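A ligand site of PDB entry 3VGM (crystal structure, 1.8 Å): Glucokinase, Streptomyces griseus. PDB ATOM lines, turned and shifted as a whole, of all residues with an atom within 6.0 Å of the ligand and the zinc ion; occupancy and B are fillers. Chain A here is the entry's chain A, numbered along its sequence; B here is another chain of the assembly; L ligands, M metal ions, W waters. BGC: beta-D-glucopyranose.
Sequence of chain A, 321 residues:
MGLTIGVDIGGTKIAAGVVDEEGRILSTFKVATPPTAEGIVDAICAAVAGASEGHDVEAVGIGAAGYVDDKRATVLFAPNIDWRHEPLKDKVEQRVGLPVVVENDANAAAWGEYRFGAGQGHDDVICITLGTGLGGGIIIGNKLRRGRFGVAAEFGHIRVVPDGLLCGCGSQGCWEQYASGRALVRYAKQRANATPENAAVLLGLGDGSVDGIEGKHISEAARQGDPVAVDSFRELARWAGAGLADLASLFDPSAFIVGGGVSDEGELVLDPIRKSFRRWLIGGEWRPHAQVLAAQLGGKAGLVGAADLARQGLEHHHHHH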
ATOM      1  N   ALA A  64     -18.387 -23.794  11.939  1.00  0.00           N
ATOM      2  CA  ALA A  64     -17.482 -22.899  11.186  1.00  0.00           C
ATOM      3  C   ALA A  64     -16.844 -21.883  12.121  1.00  0.00           C
ATOM      4  O   ALA A  64     -17.560 -21.281  12.943  1.00  0.00           O
ATOM      5  CB  ALA A  64     -18.265 -22.173  10.107  1.00  0.00           C
ATOM      6  N   ALA A  65     -15.531 -21.643  11.999  1.00  0.00           N
ATOM      7  CA  ALA A  65     -14.893 -20.539  12.740  1.00  0.00           C
ATOM      8  C   ALA A  65     -15.481 -19.210  12.240  1.00  0.00           C
ATOM      9  O   ALA A  65     -15.715 -19.046  11.040  1.00  0.00           O
ATOM     10  CB  ALA A  65     -13.353 -20.542  12.553  1.00  0.00           C
ATOM     11  N   GLY A  66     -15.748 -18.277  13.134  1.00  0.00           N
ATOM     12  CA  GLY A  66     -16.249 -16.963  12.730  1.00  0.00           C
ATOM     13  C   GLY A  66     -17.623 -16.698  13.311  1.00  0.00           C
ATOM     14  O   GLY A  66     -18.108 -17.464  14.152  1.00  0.00           O
ATOM     15  N   TYR A  67     -18.236 -15.612  12.873  1.00  0.00           N
ATOM     16  CA  TYR A  67     -19.450 -15.129  13.522  1.00  0.00           C
ATOM     17  C   TYR A  67     -20.609 -15.684  12.717  1.00  0.00           C
ATOM     18  O   TYR A  67     -20.724 -15.421  11.510  1.00  0.00           O
ATOM     19  CB  TYR A  67     -19.491 -13.576  13.565  1.00  0.00           C
ATOM     20  CG  TYR A  67     -18.157 -12.929  13.800  1.00  0.00           C
ATOM     21  CD1 TYR A  67     -17.270 -13.438  14.752  1.00  0.00           C
ATOM     22  CD2 TYR A  67     -17.777 -11.793  13.060  1.00  0.00           C
ATOM     23  CE1 TYR A  67     -16.012 -12.845  14.950  1.00  0.00           C
ATOM     24  CE2 TYR A  67     -16.531 -11.194  13.260  1.00  0.00           C
ATOM     25  CZ  TYR A  67     -15.653 -11.737  14.198  1.00  0.00           C
ATOM     26  OH  TYR A  67     -14.402 -11.191  14.376  1.00  0.00           O
ATOM     27  N   PRO A  79     -12.679 -15.915   9.810  1.00  0.00           N
ATOM     28  CA  PRO A  79     -11.315 -15.376   9.888  1.00  0.00           C
ATOM     29  C   PRO A  79     -10.346 -15.962   8.847  1.00  0.00           C
ATOM     30  O   PRO A  79      -9.347 -15.309   8.520  1.00  0.00           O
ATOM     31  CB  PRO A  79     -10.865 -15.716  11.307  1.00  0.00           C
ATOM     32  CG  PRO A  79     -11.688 -16.919  11.690  1.00  0.00           C
ATOM     33  CD  PRO A  79     -13.028 -16.725  10.998  1.00  0.00           C
ATOM     34  N   ASN A 104     -21.408 -21.649  15.058  1.00  0.00           N
ATOM     35  CA  ASN A 104     -20.004 -21.342  15.334  1.00  0.00           C
ATOM     36  C   ASN A 104     -19.249 -22.605  15.827  1.00  0.00           C
ATOM     37  O   ASN A 104     -19.818 -23.419  16.559  1.00  0.00           O
ATOM     38  CB  ASN A 104     -19.900 -20.209  16.357  1.00  0.00           C
ATOM     39  CG  ASN A 104     -18.504 -20.066  16.934  1.00  0.00           C
ATOM     40  OD1 ASN A 104     -18.218 -20.619  17.992  1.00  0.00           O
ATOM     41  ND2 ASN A 104     -17.654 -19.306  16.254  1.00  0.00           N
ATOM     42  N   ASP A 105     -17.999 -22.765  15.407  1.00  0.00           N
ATOM     43  CA  ASP A 105     -17.233 -24.013  15.681  1.00  0.00           C
ATOM     44  C   ASP A 105     -17.063 -24.283  17.160  1.00  0.00           C
ATOM     45  O   ASP A 105     -17.218 -25.420  17.604  1.00  0.00           O
ATOM     46  CB  ASP A 105     -15.881 -24.006  14.956  1.00  0.00           C
ATOM     47  CG  ASP A 105     -14.940 -22.874  15.427  1.00  0.00           C
ATOM     48  OD1 ASP A 105     -15.410 -21.820  15.885  1.00  0.00           O
ATOM     49  OD2 ASP A 105     -13.710 -23.053  15.329  1.00  0.00           O
ATOM     50  N   ALA A 106     -16.775 -23.229  17.935  1.00  0.00           N
ATOM     51  CA  ALA A 106     -16.531 -23.416  19.363  1.00  0.00           C
ATOM     52  C   ALA A 106     -17.838 -23.558  20.145  1.00  0.00           C
ATOM     53  O   ALA A 106     -17.875 -24.222  21.188  1.00  0.00           O
ATOM     54  CB  ALA A 106     -15.652 -22.285  19.932  1.00  0.00           C
ATOM     55  N   ASN A 107     -18.918 -22.940  19.646  1.00  0.00           N
ATOM     56  CA  ASN A 107     -20.256 -23.244  20.179  1.00  0.00           C
ATOM     57  C   ASN A 107     -20.563 -24.730  20.019  1.00  0.00           C
ATOM     58  O   ASN A 107     -21.047 -25.387  20.968  1.00  0.00           O
ATOM     59  CB  ASN A 107     -21.372 -22.447  19.460  1.00  0.00           C
ATOM     60  CG  ASN A 107     -21.446 -20.985  19.884  1.00  0.00           C
ATOM     61  OD1 ASN A 107     -20.761 -20.543  20.807  1.00  0.00           O
ATOM     62  ND2 ASN A 107     -22.299 -20.222  19.200  1.00  0.00           N
ATOM     63  N   THR A 129     -11.802 -23.077  24.038  1.00  0.00           N
ATOM     64  CA  THR A 129     -10.938 -23.835  23.148  1.00  0.00           C
ATOM     65  C   THR A 129      -9.685 -23.018  22.895  1.00  0.00           C
ATOM     66  O   THR A 129      -9.752 -21.932  22.313  1.00  0.00           O
ATOM     67  CB  THR A 129     -11.640 -24.124  21.794  1.00  0.00           C
ATOM     68  OG1 THR A 129     -12.895 -24.764  22.046  1.00  0.00           O
ATOM     69  CG2 THR A 129     -10.777 -25.067  20.959  1.00  0.00           C
ATOM     70  N   GLY A 133      -6.808 -20.512  16.958  1.00  0.00           N
ATOM     71  CA  GLY A 133      -7.585 -19.375  17.418  1.00  0.00           C
ATOM     72  C   GLY A 133      -8.100 -19.685  18.804  1.00  0.00           C
ATOM     73  O   GLY A 133      -7.927 -20.808  19.317  1.00  0.00           O
ATOM     74  N   LEU A 134      -8.754 -18.708  19.439  1.00  0.00           N
ATOM     75  CA  LEU A 134      -9.262 -18.962  20.767  1.00  0.00           C
ATOM     76  C   LEU A 134     -10.776 -18.779  20.673  1.00  0.00           C
ATOM     77  O   LEU A 134     -11.243 -17.755  20.199  1.00  0.00           O
ATOM     78  CB  LEU A 134      -8.660 -17.950  21.781  1.00  0.00           C
ATOM     79  CG  LEU A 134      -8.838 -18.321  23.249  1.00  0.00           C
ATOM     80  CD1 LEU A 134      -7.827 -17.489  24.091  1.00  0.00           C
ATOM     81  CD2 LEU A 134     -10.266 -18.073  23.727  1.00  0.00           C
ATOM     82  N   GLY A 135     -11.538 -19.788  21.069  1.00  0.00           N
ATOM     83  CA  GLY A 135     -12.993 -19.671  21.036  1.00  0.00           C
ATOM     84  C   GLY A 135     -13.605 -20.218  22.303  1.00  0.00           C
ATOM     85  O   GLY A 135     -12.900 -20.654  23.237  1.00  0.00           O
ATOM     86  N   GLY A 136     -14.919 -20.183  22.358  1.00  0.00           N
ATOM     87  CA  GLY A 136     -15.604 -20.845  23.475  1.00  0.00           C
ATOM     88  C   GLY A 136     -17.087 -20.917  23.244  1.00  0.00           C
ATOM     89  O   GLY A 136     -17.573 -20.566  22.160  1.00  0.00           O
ATOM     90  N   ALA A 153     -20.071 -15.359  22.940  1.00  0.00           N
ATOM     91  CA  ALA A 153     -18.930 -16.229  23.229  1.00  0.00           C
ATOM     92  C   ALA A 153     -17.833 -16.088  22.155  1.00  0.00           C
ATOM     93  O   ALA A 153     -17.152 -17.079  21.821  1.00  0.00           O
ATOM     94  CB  ALA A 153     -19.369 -17.725  23.393  1.00  0.00           C
ATOM     95  N   GLU A 154     -17.628 -14.871  21.658  1.00  0.00           N
ATOM     96  CA  GLU A 154     -16.365 -14.586  20.946  1.00  0.00           C
ATOM     97  C   GLU A 154     -15.262 -14.260  21.975  1.00  0.00           C
ATOM     98  O   GLU A 154     -14.696 -13.152  22.002  1.00  0.00           O
ATOM     99  CB  GLU A 154     -16.530 -13.457  19.917  1.00  0.00           C
ATOM    100  CG  GLU A 154     -17.206 -14.004  18.600  1.00  0.00           C
ATOM    101  CD  GLU A 154     -16.321 -15.055  17.902  1.00  0.00           C
ATOM    102  OE1 GLU A 154     -15.077 -14.916  17.912  1.00  0.00           O
ATOM    103  OE2 GLU A 154     -16.867 -16.021  17.315  1.00  0.00           O
ATOM    104  N   GLY A 156     -12.246 -15.143  22.205  1.00  0.00           N
ATOM    105  CA  GLY A 156     -10.929 -14.831  21.663  1.00  0.00           C
ATOM    106  C   GLY A 156     -10.721 -13.347  21.451  1.00  0.00           C
ATOM    107  O   GLY A 156      -9.582 -12.914  21.374  1.00  0.00           O
ATOM    108  N   HIS A 157     -11.806 -12.575  21.341  1.00  0.00           N
ATOM    109  CA  HIS A 157     -11.682 -11.164  20.985  1.00  0.00           C
ATOM    110  C   HIS A 157     -12.103 -10.188  22.075  1.00  0.00           C
ATOM    111  O   HIS A 157     -12.351  -9.001  21.799  1.00  0.00           O
ATOM    112  CB  HIS A 157     -12.357 -10.917  19.623  1.00  0.00           C
ATOM    113  CG  HIS A 157     -11.862 -11.881  18.583  1.00  0.00           C
ATOM    114  ND1 HIS A 157     -10.589 -11.802  18.056  1.00  0.00           N
ATOM    115  CD2 HIS A 157     -12.411 -13.025  18.072  1.00  0.00           C
ATOM    116  CE1 HIS A 157     -10.392 -12.807  17.206  1.00  0.00           C
ATOM    117  NE2 HIS A 157     -11.475 -13.577  17.220  1.00  0.00           N
ATOM    118  N   CYS A 167      -4.901  -7.939  15.955  1.00  0.00           N
ATOM    119  CA  CYS A 167      -5.519  -9.254  15.821  1.00  0.00           C
ATOM    120  C   CYS A 167      -6.164  -9.416  14.434  1.00  0.00           C
ATOM    121  O   CYS A 167      -6.486  -8.424  13.775  1.00  0.00           O
ATOM    122  CB  CYS A 167      -6.585  -9.383  16.914  1.00  0.00           C
ATOM    123  SG  CYS A 167      -7.457 -11.003  16.992  1.00  0.00           S
ATOM    124  N   GLY A 168      -6.327 -10.660  13.983  1.00  0.00           N
ATOM    125  CA  GLY A 168      -7.002 -10.939  12.721  1.00  0.00           C
ATOM    126  C   GLY A 168      -8.431 -10.423  12.660  1.00  0.00           C
ATOM    127  O   GLY A 168      -8.970 -10.205  11.551  1.00  0.00           O
ATOM    128  N   CYS A 169      -9.075 -10.228  13.815  1.00  0.00           N
ATOM    129  CA  CYS A 169     -10.442  -9.665  13.825  1.00  0.00           C
ATOM    130  C   CYS A 169     -10.507  -8.201  13.406  1.00  0.00           C
ATOM    131  O   CYS A 169     -11.598  -7.699  13.109  1.00  0.00           O
ATOM    132  CB  CYS A 169     -11.109  -9.851  15.190  1.00  0.00           C
ATOM    133  SG  CYS A 169     -10.499  -8.693  16.446  1.00  0.00           S
ATOM    134  N   GLY A 170      -9.368  -7.518  13.395  1.00  0.00           N
ATOM    135  CA  GLY A 170      -9.312  -6.097  13.073  1.00  0.00           C
ATOM    136  C   GLY A 170      -9.040  -5.200  14.282  1.00  0.00           C
ATOM    137  O   GLY A 170      -8.765  -4.017  14.128  1.00  0.00           O
ATOM    138  N   SER A 171      -9.136  -5.756  15.494  1.00  0.00           N
ATOM    139  CA  SER A 171      -8.970  -4.964  16.707  1.00  0.00           C
ATOM    140  C   SER A 171      -7.560  -5.154  17.296  1.00  0.00           C
ATOM    141  O   SER A 171      -6.654  -5.653  16.609  1.00  0.00           O
ATOM    142  CB  SER A 171     -10.044  -5.328  17.752  1.00  0.00           C
ATOM    143  OG  SER A 171     -10.152  -4.284  18.714  1.00  0.00           O
ATOM    144  N   GLN A 172      -7.396  -4.748  18.569  1.00  0.00           N
ATOM    145  CA  GLN A 172      -6.127  -4.843  19.282  1.00  0.00           C
ATOM    146  C   GLN A 172      -6.299  -5.470  20.649  1.00  0.00           C
ATOM    147  O   GLN A 172      -7.294  -5.197  21.341  1.00  0.00           O
ATOM    148  CB  GLN A 172      -5.561  -3.454  19.576  1.00  0.00           C
ATOM    149  CG  GLN A 172      -4.745  -2.880  18.444  1.00  0.00           C
ATOM    150  CD  GLN A 172      -4.211  -1.505  18.819  1.00  0.00           C
ATOM    151  OE1 GLN A 172      -4.751  -0.494  18.358  1.00  0.00           O
ATOM    152  NE2 GLN A 172      -3.162  -1.445  19.642  1.00  0.00           N
ATOM    153  N   CYS A 174      -6.572  -8.505  21.829  1.00  0.00           N
ATOM    154  CA  CYS A 174      -7.467  -9.666  22.035  1.00  0.00           C
ATOM    155  C   CYS A 174      -6.819 -10.839  22.788  1.00  0.00           C
ATOM    156  O   CYS A 174      -5.638 -11.171  22.601  1.00  0.00           O
ATOM    157  CB  CYS A 174      -7.936 -10.182  20.654  1.00  0.00           C
ATOM    158  SG  CYS A 174      -8.885  -8.911  19.798  1.00  0.00           S
ATOM    159  N   GLU A 176      -7.019 -13.879  22.267  1.00  0.00           N
ATOM    160  CA  GLU A 176      -6.464 -14.822  21.300  1.00  0.00           C
ATOM    161  C   GLU A 176      -5.008 -14.525  20.942  1.00  0.00           C
ATOM    162  O   GLU A 176      -4.250 -15.438  20.642  1.00  0.00           O
ATOM    163  CB  GLU A 176      -7.337 -14.775  20.019  1.00  0.00           C
ATOM    164  CG  GLU A 176      -6.777 -15.518  18.829  1.00  0.00           C
ATOM    165  CD  GLU A 176      -7.823 -15.627  17.717  1.00  0.00           C
ATOM    166  OE1 GLU A 176      -8.825 -16.339  17.944  1.00  0.00           O
ATOM    167  OE2 GLU A 176      -7.659 -14.975  16.678  1.00  0.00           O
ATOM    168  N   GLN A 177      -4.586 -13.250  21.030  1.00  0.00           N
ATOM    169  CA  GLN A 177      -3.200 -12.893  20.751  1.00  0.00           C
ATOM    170  C   GLN A 177      -2.243 -13.318  21.871  1.00  0.00           C
ATOM    171  O   GLN A 177      -1.033 -13.284  21.661  1.00  0.00           O
ATOM    172  CB  GLN A 177      -3.051 -11.377  20.521  1.00  0.00           C
ATOM    173  CG  GLN A 177      -3.719 -10.926  19.187  1.00  0.00           C
ATOM    174  CD  GLN A 177      -3.267 -11.773  18.001  1.00  0.00           C
ATOM    175  OE1 GLN A 177      -2.064 -11.937  17.784  1.00  0.00           O
ATOM    176  NE2 GLN A 177      -4.243 -12.307  17.208  1.00  0.00           N
ATOM    177  N   ARG A 182      -0.904 -19.643  18.502  1.00  0.00           N
ATOM    178  CA  ARG A 182      -0.022 -18.647  17.871  1.00  0.00           C
ATOM    179  C   ARG A 182       0.769 -17.813  18.896  1.00  0.00           C
ATOM    180  O   ARG A 182       1.944 -17.474  18.663  1.00  0.00           O
ATOM    181  CB  ARG A 182      -0.809 -17.716  16.946  1.00  0.00           C
ATOM    182  CG  ARG A 182      -1.460 -18.473  15.712  1.00  0.00           C
ATOM    183  CD  ARG A 182      -1.902 -17.442  14.629  1.00  0.00           C
ATOM    184  NE  ARG A 182      -3.182 -17.753  13.966  1.00  0.00           N
ATOM    185  CZ  ARG A 182      -4.406 -17.506  14.461  1.00  0.00           C
ATOM    186  NH1 ARG A 182      -4.586 -16.961  15.683  1.00  0.00           N
ATOM    187  NH2 ARG A 182      -5.480 -17.842  13.742  1.00  0.00           N
ATOM    188  N   ILE B 282     -15.712  -5.665  18.146  1.00  0.00           N
ATOM    189  CA  ILE B 282     -14.967  -6.514  17.185  1.00  0.00           C
ATOM    190  C   ILE B 282     -15.948  -7.046  16.162  1.00  0.00           C
ATOM    191  O   ILE B 282     -17.093  -7.408  16.494  1.00  0.00           O
ATOM    192  CB  ILE B 282     -14.125  -7.626  17.874  1.00  0.00           C
ATOM    193  CG1 ILE B 282     -15.023  -8.685  18.522  1.00  0.00           C
ATOM    194  CG2 ILE B 282     -13.130  -7.039  18.933  1.00  0.00           C
ATOM    195  CD1 ILE B 282     -15.194  -9.955  17.591  1.00  0.00           C
HETATM  196  C2  BGC L   1     -12.995 -16.843  15.895  1.00  0.00           C
HETATM  197  C3  BGC L   1     -14.059 -17.729  16.548  1.00  0.00           C
HETATM  198  C4  BGC L   1     -13.636 -19.199  16.585  1.00  0.00           C
HETATM  199  C5  BGC L   1     -12.201 -19.348  17.117  1.00  0.00           C
HETATM  200  C6  BGC L   1     -11.717 -20.805  17.061  1.00  0.00           C
HETATM  201  C1  BGC L   1     -11.651 -17.153  16.589  1.00  0.00           C
HETATM  202  O1  BGC L   1     -10.627 -16.398  16.037  1.00  0.00           O
HETATM  203  O2  BGC L   1     -13.322 -15.464  16.028  1.00  0.00           O
HETATM  204  O3  BGC L   1     -15.305 -17.572  15.912  1.00  0.00           O
HETATM  205  O4  BGC L   1     -14.537 -19.935  17.417  1.00  0.00           O
HETATM  206  O5  BGC L   1     -11.330 -18.519  16.330  1.00  0.00           O
HETATM  207  O6  BGC L   1     -11.727 -21.238  15.706  1.00  0.00           O
HETATM  208 ZN    ZN M   1      -9.389 -10.140  17.921  1.00  0.00          ZN
HETATM  209  O   HOH W   1      -9.784 -22.817  18.938  1.00  0.00           O
HETATM  210  O   HOH W   2     -12.548 -13.585  13.974  1.00  0.00           O
HETATM  211  O   HOH W   3      -8.703 -22.737  16.387  1.00  0.00           O
HETATM  212  O   HOH W   4     -15.765 -18.795  19.658  1.00  0.00           O
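O2 of the ligand sits at hydrogen-bond distance from NE2 of His 157, at 2.9 Å.
The side-chain carboxylate (OD1) of Asp 105 sits at hydrogen-bond distance from an oxygen (O4) of the ligand (2.6 Å).
The side-chain carboxylate (OE2) of Glu 154 lies within hydrogen-bond range of an oxygen (O3) of the ligand, at 2.6 Å.
OE1 of Glu 176 is in hydrogen-bond range of O1 of the ligand.
The backbone NH (N) of Gly 66 sits at hydrogen-bond distance from an oxygen (O3) of the ligand, at 2.9 Å.
An oxygen (O3) of the ligand lies within hydrogen-bond range of the backbone carbonyl oxygen of Gly 66.
The side-chain amide nitrogen of Asn 104 is in hydrogen-bond range of an oxygen (O3) of the ligand (2.9 Å).
N of Ser 171 sits close to SG of Cys 169, 3.4 Å away.
The side-chain carboxylate (OD1) of Asp 105 sits at hydrogen-bond distance from the side-chain amide nitrogen (ND2) of Asn 104 (3.4 Å).
The backbone NH (N) of Asp 105 sits at hydrogen-bond distance from the backbone carbonyl oxygen (O) of Ala 64 (2.9 Å).
The backbone NH (N) of Glu 176 sits at hydrogen-bond distance from the backbone carbonyl oxygen (O) of Gly 156 (2.9 Å).
The side-chain carboxylate of Glu 176 is in salt-bridge range of the guanidinium group of Arg 182.
O of Gly 66 is in hydrogen-bond range of ND2 of Asn 104, 2.8 Å away.
N of Ala 106 sits at hydrogen-bond distance from OD1 of Asn 104, at 3.0 Å.
N of Thr 129 lies within hydrogen-bond range of O of Gly 135 (2.8 Å).
Ala 65 touches the ligand.
CE1 of Tyr 67 touches O2 of the ligand, 3.9 Å away.
Ala 106 touches the ligand (CB to O4, 3.6 Å).
Gly 133 touches the ligand (CA to O5, 3.99 Å).
O of Leu 134 touches C5 of the ligand (3.6 Å).
Gly 135 touches the ligand (CA to O4, 3.9 Å).
Hydrophobic or aromatic side chains within 4 Å of the ligand: Ala 65, Tyr 67, Ala 106 and His 157.
The nearest printed residue that does not touch the ligand is Pro 79 (4.4 Å).
Within 4 Å of the zinc ion: His 157, Cys 167, Cys 169 and Cys 174.
The nearest printed residue that does not touch the zinc ion is Gly 156 (4.4 Å).
The zinc ion is bound by ND1 of His 157 (2.1 Å), SG of Cys 174 (2.3 Å), SG of Cys 167 (2.3 Å) and SG of Cys 169 (2.3 Å).
The zinc ion has four donor atoms within binding distance.
Water W4 lies within hydrogen-bond range of O4 of the ligand, O of Ala 153, N of Gly 136 and OD1 of Asn 104.
Water W2 lies within hydrogen-bond range of an oxygen (O2) of the ligand, the side-chain hydroxyl of Tyr 67 and a ring nitrogen (NE2) of His 157.
Water W3 lies within hydrogen-bond range of the backbone NH of Gly 133 (3.0 Å) and an oxygen (O6) of the ligand (3.4 Å).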
